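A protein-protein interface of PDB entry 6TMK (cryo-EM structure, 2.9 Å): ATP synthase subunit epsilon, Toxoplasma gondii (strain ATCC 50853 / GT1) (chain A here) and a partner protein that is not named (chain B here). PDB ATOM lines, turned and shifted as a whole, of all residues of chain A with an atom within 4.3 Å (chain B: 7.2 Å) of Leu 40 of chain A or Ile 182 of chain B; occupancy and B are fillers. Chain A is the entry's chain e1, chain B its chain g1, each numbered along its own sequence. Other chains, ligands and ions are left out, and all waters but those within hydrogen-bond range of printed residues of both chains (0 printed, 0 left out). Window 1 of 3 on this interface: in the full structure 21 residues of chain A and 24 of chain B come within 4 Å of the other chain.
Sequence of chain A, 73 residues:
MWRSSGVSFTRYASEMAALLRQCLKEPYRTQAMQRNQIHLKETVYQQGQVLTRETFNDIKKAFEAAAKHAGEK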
ATOM      1  N   ILE A  38      11.004 -24.435  13.864  1.00  0.00           N
ATOM      2  CA  ILE A  38      11.381 -23.339  14.754  1.00  0.00           C
ATOM      3  C   ILE A  38      10.402 -23.277  15.919  1.00  0.00           C
ATOM      4  O   ILE A  38       9.196 -23.482  15.745  1.00  0.00           O
ATOM      5  CB  ILE A  38      11.428 -21.988  14.012  1.00  0.00           C
ATOM      6  CG1 ILE A  38      12.531 -22.000  12.955  1.00  0.00           C
ATOM      7  CG2 ILE A  38      11.669 -20.858  14.994  1.00  0.00           C
ATOM      8  CD1 ILE A  38      12.429 -20.877  11.957  1.00  0.00           C
ATOM      9  N   HIS A  39      10.928 -22.992  17.112  1.00  0.00           N
ATOM     10  CA  HIS A  39      10.091 -22.725  18.282  1.00  0.00           C
ATOM     11  C   HIS A  39      10.888 -21.896  19.282  1.00  0.00           C
ATOM     12  O   HIS A  39      11.805 -22.418  19.920  1.00  0.00           O
ATOM     13  CB  HIS A  39       9.610 -24.020  18.916  1.00  0.00           C
ATOM     14  CG  HIS A  39       8.715 -23.810  20.096  1.00  0.00           C
ATOM     15  ND1 HIS A  39       7.796 -22.784  20.157  1.00  0.00           N
ATOM     16  CD2 HIS A  39       8.606 -24.482  21.265  1.00  0.00           C
ATOM     17  CE1 HIS A  39       7.157 -22.838  21.311  1.00  0.00           C
ATOM     18  NE2 HIS A  39       7.628 -23.860  22.001  1.00  0.00           N
ATOM     19  N   LEU A  40      10.539 -20.616  19.414  1.00  0.00           N
ATOM     20  CA  LEU A  40      11.199 -19.727  20.360  1.00  0.00           C
ATOM     21  C   LEU A  40      10.158 -18.881  21.077  1.00  0.00           C
ATOM     22  O   LEU A  40       9.012 -18.771  20.642  1.00  0.00           O
ATOM     23  CB  LEU A  40      12.216 -18.810  19.671  1.00  0.00           C
ATOM     24  CG  LEU A  40      13.290 -19.499  18.830  1.00  0.00           C
ATOM     25  CD1 LEU A  40      13.826 -18.553  17.772  1.00  0.00           C
ATOM     26  CD2 LEU A  40      14.413 -19.989  19.722  1.00  0.00           C
ATOM     27  N   LYS A  41      10.573 -18.284  22.194  1.00  0.00           N
ATOM     28  CA  LYS A  41       9.692 -17.442  23.007  1.00  0.00           C
ATOM     29  C   LYS A  41      10.512 -16.275  23.548  1.00  0.00           C
ATOM     30  O   LYS A  41      11.176 -16.400  24.581  1.00  0.00           O
ATOM     31  CB  LYS A  41       9.050 -18.232  24.136  1.00  0.00           C
ATOM     32  CG  LYS A  41       8.274 -17.361  25.098  1.00  0.00           C
ATOM     33  CD  LYS A  41       7.342 -18.175  25.970  1.00  0.00           C
ATOM     34  CE  LYS A  41       6.586 -17.283  26.940  1.00  0.00           C
ATOM     35  NZ  LYS A  41       5.261 -17.853  27.306  1.00  0.00           N
ATOM     36  N   GLU A  42      10.456 -15.145  22.851  1.00  0.00           N
ATOM     37  CA  GLU A  42      11.173 -13.952  23.265  1.00  0.00           C
ATOM     38  C   GLU A  42      10.437 -13.238  24.394  1.00  0.00           C
ATOM     39  O   GLU A  42       9.203 -13.215  24.450  1.00  0.00           O
ATOM     40  CB  GLU A  42      11.360 -13.006  22.079  1.00  0.00           C
ATOM     41  CG  GLU A  42      12.354 -11.882  22.320  1.00  0.00           C
ATOM     42  CD  GLU A  42      12.252 -10.779  21.284  1.00  0.00           C
ATOM     43  OE1 GLU A  42      11.460 -10.926  20.331  1.00  0.00           O
ATOM     44  OE2 GLU A  42      12.968  -9.764  21.422  1.00  0.00           O
ATOM     45  N   THR A  55       5.765 -15.494  21.116  1.00  0.00           N
ATOM     46  CA  THR A  55       6.254 -16.759  20.600  1.00  0.00           C
ATOM     47  C   THR A  55       6.552 -16.628  19.112  1.00  0.00           C
ATOM     48  O   THR A  55       6.028 -15.751  18.420  1.00  0.00           O
ATOM     49  CB  THR A  55       5.234 -17.873  20.830  1.00  0.00           C
ATOM     50  OG1 THR A  55       3.959 -17.473  20.315  1.00  0.00           O
ATOM     51  CG2 THR A  55       5.103 -18.171  22.309  1.00  0.00           C
ATOM     52  N   PHE A  56       7.407 -17.521  18.626  1.00  0.00           N
ATOM     53  CA  PHE A  56       7.797 -17.543  17.227  1.00  0.00           C
ATOM     54  C   PHE A  56       7.904 -18.984  16.762  1.00  0.00           C
ATOM     55  O   PHE A  56       8.573 -19.799  17.405  1.00  0.00           O
ATOM     56  CB  PHE A  56       9.133 -16.827  17.015  1.00  0.00           C
ATOM     57  CG  PHE A  56       9.123 -15.389  17.431  1.00  0.00           C
ATOM     58  CD1 PHE A  56       8.248 -14.492  16.849  1.00  0.00           C
ATOM     59  CD2 PHE A  56      10.004 -14.931  18.395  1.00  0.00           C
ATOM     60  CE1 PHE A  56       8.242 -13.167  17.231  1.00  0.00           C
ATOM     61  CE2 PHE A  56      10.003 -13.608  18.777  1.00  0.00           C
ATOM     62  CZ  PHE A  56       9.122 -12.724  18.193  1.00  0.00           C
ATOM     63  N   ILE A  59      10.452 -18.427  10.610  1.00  0.00           N
ATOM     64  CA  ILE A  59      11.708 -17.696  10.493  1.00  0.00           C
ATOM     65  C   ILE A  59      11.442 -16.237  10.149  1.00  0.00           C
ATOM     66  O   ILE A  59      12.069 -15.328  10.708  1.00  0.00           O
ATOM     67  CB  ILE A  59      12.614 -18.381   9.452  1.00  0.00           C
ATOM     68  CG1 ILE A  59      14.031 -17.813   9.513  1.00  0.00           C
ATOM     69  CG2 ILE A  59      12.036 -18.237   8.052  1.00  0.00           C
ATOM     70  CD1 ILE A  59      14.788 -18.234  10.747  1.00  0.00           C
ATOM     71  N   ALA A  62       9.945 -14.359  13.001  1.00  0.00           N
ATOM     72  CA  ALA A  62      10.933 -14.271  14.068  1.00  0.00           C
ATOM     73  C   ALA A  62      11.940 -13.172  13.779  1.00  0.00           C
ATOM     74  O   ALA A  62      12.337 -12.429  14.683  1.00  0.00           O
ATOM     75  CB  ALA A  62      11.635 -15.614  14.247  1.00  0.00           C
ATOM     76  N   PHE A  63      12.362 -13.048  12.520  1.00  0.00           N
ATOM     77  CA  PHE A  63      13.307 -11.997  12.170  1.00  0.00           C
ATOM     78  C   PHE A  63      12.618 -10.645  12.085  1.00  0.00           C
ATOM     79  O   PHE A  63      13.244  -9.615  12.354  1.00  0.00           O
ATOM     80  CB  PHE A  63      13.987 -12.322  10.843  1.00  0.00           C
ATOM     81  CG  PHE A  63      15.160 -13.243  10.972  1.00  0.00           C
ATOM     82  CD1 PHE A  63      15.173 -14.458  10.318  1.00  0.00           C
ATOM     83  CD2 PHE A  63      16.258 -12.884  11.730  1.00  0.00           C
ATOM     84  CE1 PHE A  63      16.253 -15.304  10.429  1.00  0.00           C
ATOM     85  CE2 PHE A  63      17.340 -13.727  11.844  1.00  0.00           C
ATOM     86  CZ  PHE A  63      17.338 -14.939  11.195  1.00  0.00           C
ATOM     87  N   MET B 167      15.478 -15.472  25.933  1.00  0.00           N
ATOM     88  CA  MET B 167      14.868 -16.465  25.066  1.00  0.00           C
ATOM     89  C   MET B 167      14.746 -17.780  25.821  1.00  0.00           C
ATOM     90  O   MET B 167      15.593 -18.118  26.652  1.00  0.00           O
ATOM     91  CB  MET B 167      15.693 -16.677  23.792  1.00  0.00           C
ATOM     92  CG  MET B 167      15.951 -15.412  22.992  1.00  0.00           C
ATOM     93  SD  MET B 167      14.472 -14.799  22.167  1.00  0.00           S
ATOM     94  CE  MET B 167      14.362 -15.942  20.793  1.00  0.00           C
ATOM     95  N   THR B 168      13.683 -18.519  25.526  1.00  0.00           N
ATOM     96  CA  THR B 168      13.422 -19.784  26.197  1.00  0.00           C
ATOM     97  C   THR B 168      12.512 -20.625  25.313  1.00  0.00           C
ATOM     98  O   THR B 168      12.142 -20.224  24.206  1.00  0.00           O
ATOM     99  CB  THR B 168      12.806 -19.556  27.580  1.00  0.00           C
ATOM    100  OG1 THR B 168      12.831 -20.779  28.326  1.00  0.00           O
ATOM    101  CG2 THR B 168      11.375 -19.070  27.457  1.00  0.00           C
ATOM    102  N   GLU B 169      12.155 -21.805  25.817  1.00  0.00           N
ATOM    103  CA  GLU B 169      11.459 -22.815  25.026  1.00  0.00           C
ATOM    104  C   GLU B 169      12.247 -23.126  23.759  1.00  0.00           C
ATOM    105  O   GLU B 169      11.686 -23.383  22.692  1.00  0.00           O
ATOM    106  CB  GLU B 169      10.039 -22.364  24.686  1.00  0.00           C
ATOM    107  CG  GLU B 169       9.168 -22.097  25.898  1.00  0.00           C
ATOM    108  CD  GLU B 169       7.716 -22.446  25.655  1.00  0.00           C
ATOM    109  OE1 GLU B 169       7.120 -23.137  26.507  1.00  0.00           O
ATOM    110  OE2 GLU B 169       7.170 -22.029  24.611  1.00  0.00           O
ATOM    111  N   VAL B 170      13.571 -23.108  23.888  1.00  0.00           N
ATOM    112  CA  VAL B 170      14.442 -23.163  22.719  1.00  0.00           C
ATOM    113  C   VAL B 170      14.669 -24.606  22.290  1.00  0.00           C
ATOM    114  O   VAL B 170      14.343 -25.000  21.165  1.00  0.00           O
ATOM    115  CB  VAL B 170      15.775 -22.452  23.014  1.00  0.00           C
ATOM    116  CG1 VAL B 170      16.713 -22.572  21.832  1.00  0.00           C
ATOM    117  CG2 VAL B 170      15.531 -20.997  23.348  1.00  0.00           C
ATOM    118  N   THR B 171      15.233 -25.415  23.188  1.00  0.00           N
ATOM    119  CA  THR B 171      15.672 -26.766  22.869  1.00  0.00           C
ATOM    120  C   THR B 171      14.580 -27.805  23.087  1.00  0.00           C
ATOM    121  O   THR B 171      14.884 -28.963  23.401  1.00  0.00           O
ATOM    122  CB  THR B 171      16.910 -27.119  23.693  1.00  0.00           C
ATOM    123  OG1 THR B 171      17.737 -25.957  23.831  1.00  0.00           O
ATOM    124  CG2 THR B 171      17.712 -28.220  23.010  1.00  0.00           C
ATOM    125  N   PHE B 173      13.122 -28.838  20.525  1.00  0.00           N
ATOM    126  CA  PHE B 173      13.675 -29.600  19.416  1.00  0.00           C
ATOM    127  C   PHE B 173      15.196 -29.627  19.504  1.00  0.00           C
ATOM    128  O   PHE B 173      15.774 -29.092  20.459  1.00  0.00           O
ATOM    129  CB  PHE B 173      13.222 -29.001  18.087  1.00  0.00           C
ATOM    130  CG  PHE B 173      11.743 -28.767  18.006  1.00  0.00           C
ATOM    131  CD1 PHE B 173      11.242 -27.504  17.760  1.00  0.00           C
ATOM    132  CD2 PHE B 173      10.855 -29.813  18.172  1.00  0.00           C
ATOM    133  CE1 PHE B 173       9.882 -27.288  17.683  1.00  0.00           C
ATOM    134  CE2 PHE B 173       9.495 -29.603  18.096  1.00  0.00           C
ATOM    135  CZ  PHE B 173       9.008 -28.338  17.853  1.00  0.00           C
ATOM    136  N   TRP B 175      18.962 -28.252  18.068  1.00  0.00           N
ATOM    137  CA  TRP B 175      19.461 -26.910  18.349  1.00  0.00           C
ATOM    138  C   TRP B 175      19.109 -25.929  17.237  1.00  0.00           C
ATOM    139  O   TRP B 175      18.378 -24.959  17.464  1.00  0.00           O
ATOM    140  CB  TRP B 175      20.972 -26.962  18.570  1.00  0.00           C
ATOM    141  CG  TRP B 175      21.636 -25.624  18.561  1.00  0.00           C
ATOM    142  CD1 TRP B 175      22.842 -25.321  18.007  1.00  0.00           C
ATOM    143  CD2 TRP B 175      21.136 -24.404  19.123  1.00  0.00           C
ATOM    144  NE1 TRP B 175      23.128 -23.993  18.189  1.00  0.00           N
ATOM    145  CE2 TRP B 175      22.095 -23.406  18.870  1.00  0.00           C
ATOM    146  CE3 TRP B 175      19.971 -24.058  19.812  1.00  0.00           C
ATOM    147  CZ2 TRP B 175      21.927 -22.088  19.284  1.00  0.00           C
ATOM    148  CZ3 TRP B 175      19.808 -22.750  20.221  1.00  0.00           C
ATOM    149  CH2 TRP B 175      20.779 -21.781  19.955  1.00  0.00           C
ATOM    150  N   PHE B 177      17.122 -25.703  15.093  1.00  0.00           N
ATOM    151  CA  PHE B 177      15.725 -25.297  15.065  1.00  0.00           C
ATOM    152  C   PHE B 177      15.608 -23.821  15.424  1.00  0.00           C
ATOM    153  O   PHE B 177      15.216 -22.995  14.595  1.00  0.00           O
ATOM    154  CB  PHE B 177      14.908 -26.134  16.047  1.00  0.00           C
ATOM    155  CG  PHE B 177      14.573 -27.502  15.543  1.00  0.00           C
ATOM    156  CD1 PHE B 177      15.514 -28.516  15.592  1.00  0.00           C
ATOM    157  CD2 PHE B 177      13.314 -27.786  15.050  1.00  0.00           C
ATOM    158  CE1 PHE B 177      15.212 -29.781  15.138  1.00  0.00           C
ATOM    159  CE2 PHE B 177      13.006 -29.051  14.603  1.00  0.00           C
ATOM    160  CZ  PHE B 177      13.958 -30.048  14.641  1.00  0.00           C
ATOM    161  N   GLY B 178      15.959 -23.494  16.667  1.00  0.00           N
ATOM    162  CA  GLY B 178      15.971 -22.127  17.148  1.00  0.00           C
ATOM    163  C   GLY B 178      17.229 -21.400  16.727  1.00  0.00           C
ATOM    164  O   GLY B 178      18.141 -21.203  17.535  1.00  0.00           O
ATOM    165  N   GLN B 179      17.287 -20.996  15.461  1.00  0.00           N
ATOM    166  CA  GLN B 179      18.555 -20.629  14.851  1.00  0.00           C
ATOM    167  C   GLN B 179      19.267 -19.541  15.643  1.00  0.00           C
ATOM    168  O   GLN B 179      18.651 -18.591  16.133  1.00  0.00           O
ATOM    169  CB  GLN B 179      18.338 -20.165  13.412  1.00  0.00           C
ATOM    170  CG  GLN B 179      17.854 -21.253  12.482  1.00  0.00           C
ATOM    171  CD  GLN B 179      17.692 -20.769  11.059  1.00  0.00           C
ATOM    172  OE1 GLN B 179      17.936 -19.602  10.757  1.00  0.00           O
ATOM    173  NE2 GLN B 179      17.280 -21.667  10.173  1.00  0.00           N
ATOM    174  N   ALA B 180      20.583 -19.705  15.766  1.00  0.00           N
ATOM    175  CA  ALA B 180      21.439 -18.692  16.366  1.00  0.00           C
ATOM    176  C   ALA B 180      21.408 -17.392  15.581  1.00  0.00           C
ATOM    177  O   ALA B 180      21.747 -16.339  16.132  1.00  0.00           O
ATOM    178  CB  ALA B 180      22.872 -19.216  16.465  1.00  0.00           C
ATOM    179  N   CYS B 181      21.049 -17.455  14.298  1.00  0.00           N
ATOM    180  CA  CYS B 181      20.995 -16.257  13.470  1.00  0.00           C
ATOM    181  C   CYS B 181      20.029 -15.231  14.048  1.00  0.00           C
ATOM    182  O   CYS B 181      20.289 -14.025  13.988  1.00  0.00           O
ATOM    183  CB  CYS B 181      20.581 -16.629  12.048  1.00  0.00           C
ATOM    184  SG  CYS B 181      21.841 -17.524  11.108  1.00  0.00           S
ATOM    185  N   ILE B 182      18.921 -15.687  14.630  1.00  0.00           N
ATOM    186  CA  ILE B 182      17.952 -14.759  15.206  1.00  0.00           C
ATOM    187  C   ILE B 182      18.578 -13.995  16.365  1.00  0.00           C
ATOM    188  O   ILE B 182      18.477 -12.765  16.454  1.00  0.00           O
ATOM    189  CB  ILE B 182      16.690 -15.515  15.654  1.00  0.00           C
ATOM    190  CG1 ILE B 182      15.903 -16.005  14.442  1.00  0.00           C
ATOM    191  CG2 ILE B 182      15.822 -14.632  16.519  1.00  0.00           C
ATOM    192  CD1 ILE B 182      15.145 -17.279  14.693  1.00  0.00           C
ATOM    193  N   ILE B 183      19.219 -14.718  17.281  1.00  0.00           N
ATOM    194  CA  ILE B 183      19.829 -14.078  18.441  1.00  0.00           C
ATOM    195  C   ILE B 183      20.957 -13.150  18.005  1.00  0.00           C
ATOM    196  O   ILE B 183      21.130 -12.055  18.554  1.00  0.00           O
ATOM    197  CB  ILE B 183      20.320 -15.150  19.426  1.00  0.00           C
ATOM    198  CG1 ILE B 183      19.123 -15.845  20.070  1.00  0.00           C
ATOM    199  CG2 ILE B 183      21.209 -14.528  20.484  1.00  0.00           C
ATOM    200  CD1 ILE B 183      19.335 -17.314  20.325  1.00  0.00           C
ATOM    201  N   ALA B 184      21.741 -13.571  17.011  1.00  0.00           N
ATOM    202  CA  ALA B 184      22.820 -12.726  16.511  1.00  0.00           C
ATOM    203  C   ALA B 184      22.275 -11.441  15.903  1.00  0.00           C
ATOM    204  O   ALA B 184      22.832 -10.356  16.110  1.00  0.00           O
ATOM    205  CB  ALA B 184      23.654 -13.493  15.486  1.00  0.00           C
ATOM    206  N   ASP B 185      21.183 -11.545  15.144  1.00  0.00           N
ATOM    207  CA  ASP B 185      20.546 -10.356  14.596  1.00  0.00           C
ATOM    208  C   ASP B 185      20.031  -9.450  15.704  1.00  0.00           C
ATOM    209  O   ASP B 185      20.134  -8.223  15.606  1.00  0.00           O
ATOM    210  CB  ASP B 185      19.410 -10.761  13.661  1.00  0.00           C
ATOM    211  CG  ASP B 185      19.909 -11.214  12.302  1.00  0.00           C
ATOM    212  OD1 ASP B 185      19.078 -11.379  11.386  1.00  0.00           O
ATOM    213  OD2 ASP B 185      21.135 -11.408  12.150  1.00  0.00           O
ATOM    214  N   ARG B 186      19.453 -10.029  16.757  1.00  0.00           N
ATOM    215  CA  ARG B 186      18.999  -9.212  17.878  1.00  0.00           C
ATOM    216  C   ARG B 186      20.166  -8.489  18.543  1.00  0.00           C
ATOM    217  O   ARG B 186      20.062  -7.303  18.885  1.00  0.00           O
ATOM    218  CB  ARG B 186      18.262 -10.080  18.895  1.00  0.00           C
ATOM    219  CG  ARG B 186      16.939 -10.617  18.394  1.00  0.00           C
ATOM    220  CD  ARG B 186      15.852  -9.569  18.481  1.00  0.00           C
ATOM    221  NE  ARG B 186      14.869  -9.711  17.410  1.00  0.00           N
ATOM    222  CZ  ARG B 186      13.972 -10.688  17.348  1.00  0.00           C
ATOM    223  NH1 ARG B 186      13.930 -11.613  18.294  1.00  0.00           N
ATOM    224  NH2 ARG B 186      13.113 -10.742  16.340  1.00  0.00           N
ATOM    225  N   LEU B 187      21.316  -9.157  18.652  1.00  0.00           N
ATOM    226  CA  LEU B 187      22.488  -8.502  19.226  1.00  0.00           C
ATOM    227  C   LEU B 187      22.961  -7.362  18.338  1.00  0.00           C
ATOM    228  O   LEU B 187      23.281  -6.269  18.828  1.00  0.00           O
ATOM    229  CB  LEU B 187      23.616  -9.512  19.436  1.00  0.00           C
ATOM    230  CG  LEU B 187      23.679 -10.243  20.779  1.00  0.00           C
ATOM    231  CD1 LEU B 187      23.887  -9.259  21.914  1.00  0.00           C
ATOM    232  CD2 LEU B 187      22.439 -11.074  21.018  1.00  0.00           C
ATOM    233  N   MET B 188      22.979  -7.580  17.026  1.00  0.00           N
ATOM    234  CA  MET B 188      23.512  -6.548  16.152  1.00  0.00           C
ATOM    235  C   MET B 188      22.554  -5.369  16.122  1.00  0.00           C
ATOM    236  O   MET B 188      22.984  -4.211  16.071  1.00  0.00           O
ATOM    237  CB  MET B 188      23.760  -7.107  14.752  1.00  0.00           C
ATOM    238  CG  MET B 188      24.614  -6.201  13.881  1.00  0.00           C
ATOM    239  SD  MET B 188      26.319  -6.094  14.460  1.00  0.00           S
ATOM    240  CE  MET B 188      26.980  -7.652  13.885  1.00  0.00           C
ATOM    241  N   GLN B 189      21.249  -5.647  16.151  1.00  0.00           N
ATOM    242  CA  GLN B 189      20.271  -4.573  16.222  1.00  0.00           C
ATOM    243  C   GLN B 189      20.444  -3.802  17.520  1.00  0.00           C
ATOM    244  O   GLN B 189      20.195  -2.592  17.567  1.00  0.00           O
ATOM    245  CB  GLN B 189      18.857  -5.141  16.119  1.00  0.00           C
ATOM    246  CG  GLN B 189      18.529  -5.737  14.763  1.00  0.00           C
ATOM    247  CD  GLN B 189      17.371  -6.717  14.823  1.00  0.00           C
ATOM    248  OE1 GLN B 189      16.631  -6.760  15.805  1.00  0.00           O
ATOM    249  NE2 GLN B 189      17.219  -7.518  13.775  1.00  0.00           N
ATOM    250  N   ALA B 251      26.780 -15.573  14.331  1.00  0.00           N
ATOM    251  CA  ALA B 251      25.934 -16.764  14.301  1.00  0.00           C
ATOM    252  C   ALA B 251      26.735 -18.029  14.587  1.00  0.00           C
ATOM    253  O   ALA B 251      26.339 -18.852  15.420  1.00  0.00           O
ATOM    254  CB  ALA B 251      25.235 -16.872  12.950  1.00  0.00           C
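Printed residues of chain B that touch a printed residue of chain A: Met 167, Thr 168, Glu 169, Val 170, Phe 173, Phe 177, Gly 178, Gln 179, Cys 181, Ile 182, Asp 185 and Arg 186.
Hydrophobic or aromatic side chains of chain B that line the printed part of chain A: Met 167, Val 170, Phe 173 and Ile 182.
Printed residues of chain A that touch a printed residue of chain B: Ile 38, His 39, Leu 40, Lys 41, Glu 42, Ile 59, Ala 62 and Phe 63.
Among the printed residues, 19 pairs touch across the chains.
Among the printed residues, merely in contact across the chains: Phe 63 of chain A with Asp 185 of chain B (3.0 Å), Ile 38 of chain A with Phe 177 of chain B (3.3 Å), Ile 59 of chain A with Gln 179 of chain B (3.4 Å), His 39 of chain A with Phe 173 of chain B (3.5 Å), Phe 63 of chain A with Ile 182 of chain B (3.6 Å), Glu 42 of chain A with Met 167 of chain B (3.6 Å), Leu 40 of chain A with Ile 182 of chain B (3.6 Å), Phe 63 of chain A with Cys 181 of chain B (3.7 Å), Leu 40 of chain A with Gly 178 of chain B (3.7 Å), Lys 41 of chain A with Met 167 of chain B (3.7 Å), Leu 40 of chain A with Met 167 of chain B (3.8 Å), His 39 of chain A with Val 170 of chain B (3.8 Å), Ala 62 of chain A with Ile 182 of chain B (3.9 Å), Leu 40 of chain A with Val 170 of chain B (3.9 Å) and Leu 40 of chain A with Thr 168 of chain B (3.9 Å).
Leu 40 of chain A touches five residues of chain B.
Of the printed residues of chain B, Ile 59 of chain A touches Gln 179 (3.4 Å).
Printed residues of chain A within 4 Å of Phe 173 of chain B: His 39 (3.5 Å).
Of chain A, only Leu 40, Ala 62 and Phe 63 come within 4 Å of Ile 182 of chain B.
The guanidinium group of Arg 186 of chain B lies within salt-bridge range of the side-chain carboxylate of Glu 42 of chain A, 3.3 Å away.
NE2 of His 39 of chain A sits at hydrogen-bond distance from OE2 of Glu 169 of chain B (3.2 Å).
The backbone carbonyl oxygen (O) of Ala 62 of chain A lies within hydrogen-bond range of the guanidinium group (NH2) of Arg 186 of chain B (2.5 Å).
O of Thr 168 of chain B sits at hydrogen-bond distance from N of Lys 41 of chain A (3.2 Å).
The backbone carbonyl oxygen (O) of Leu 40 of chain A is in hydrogen-bond range of the backbone NH (N) of Phe 56 of chain A, at 2.9 Å.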
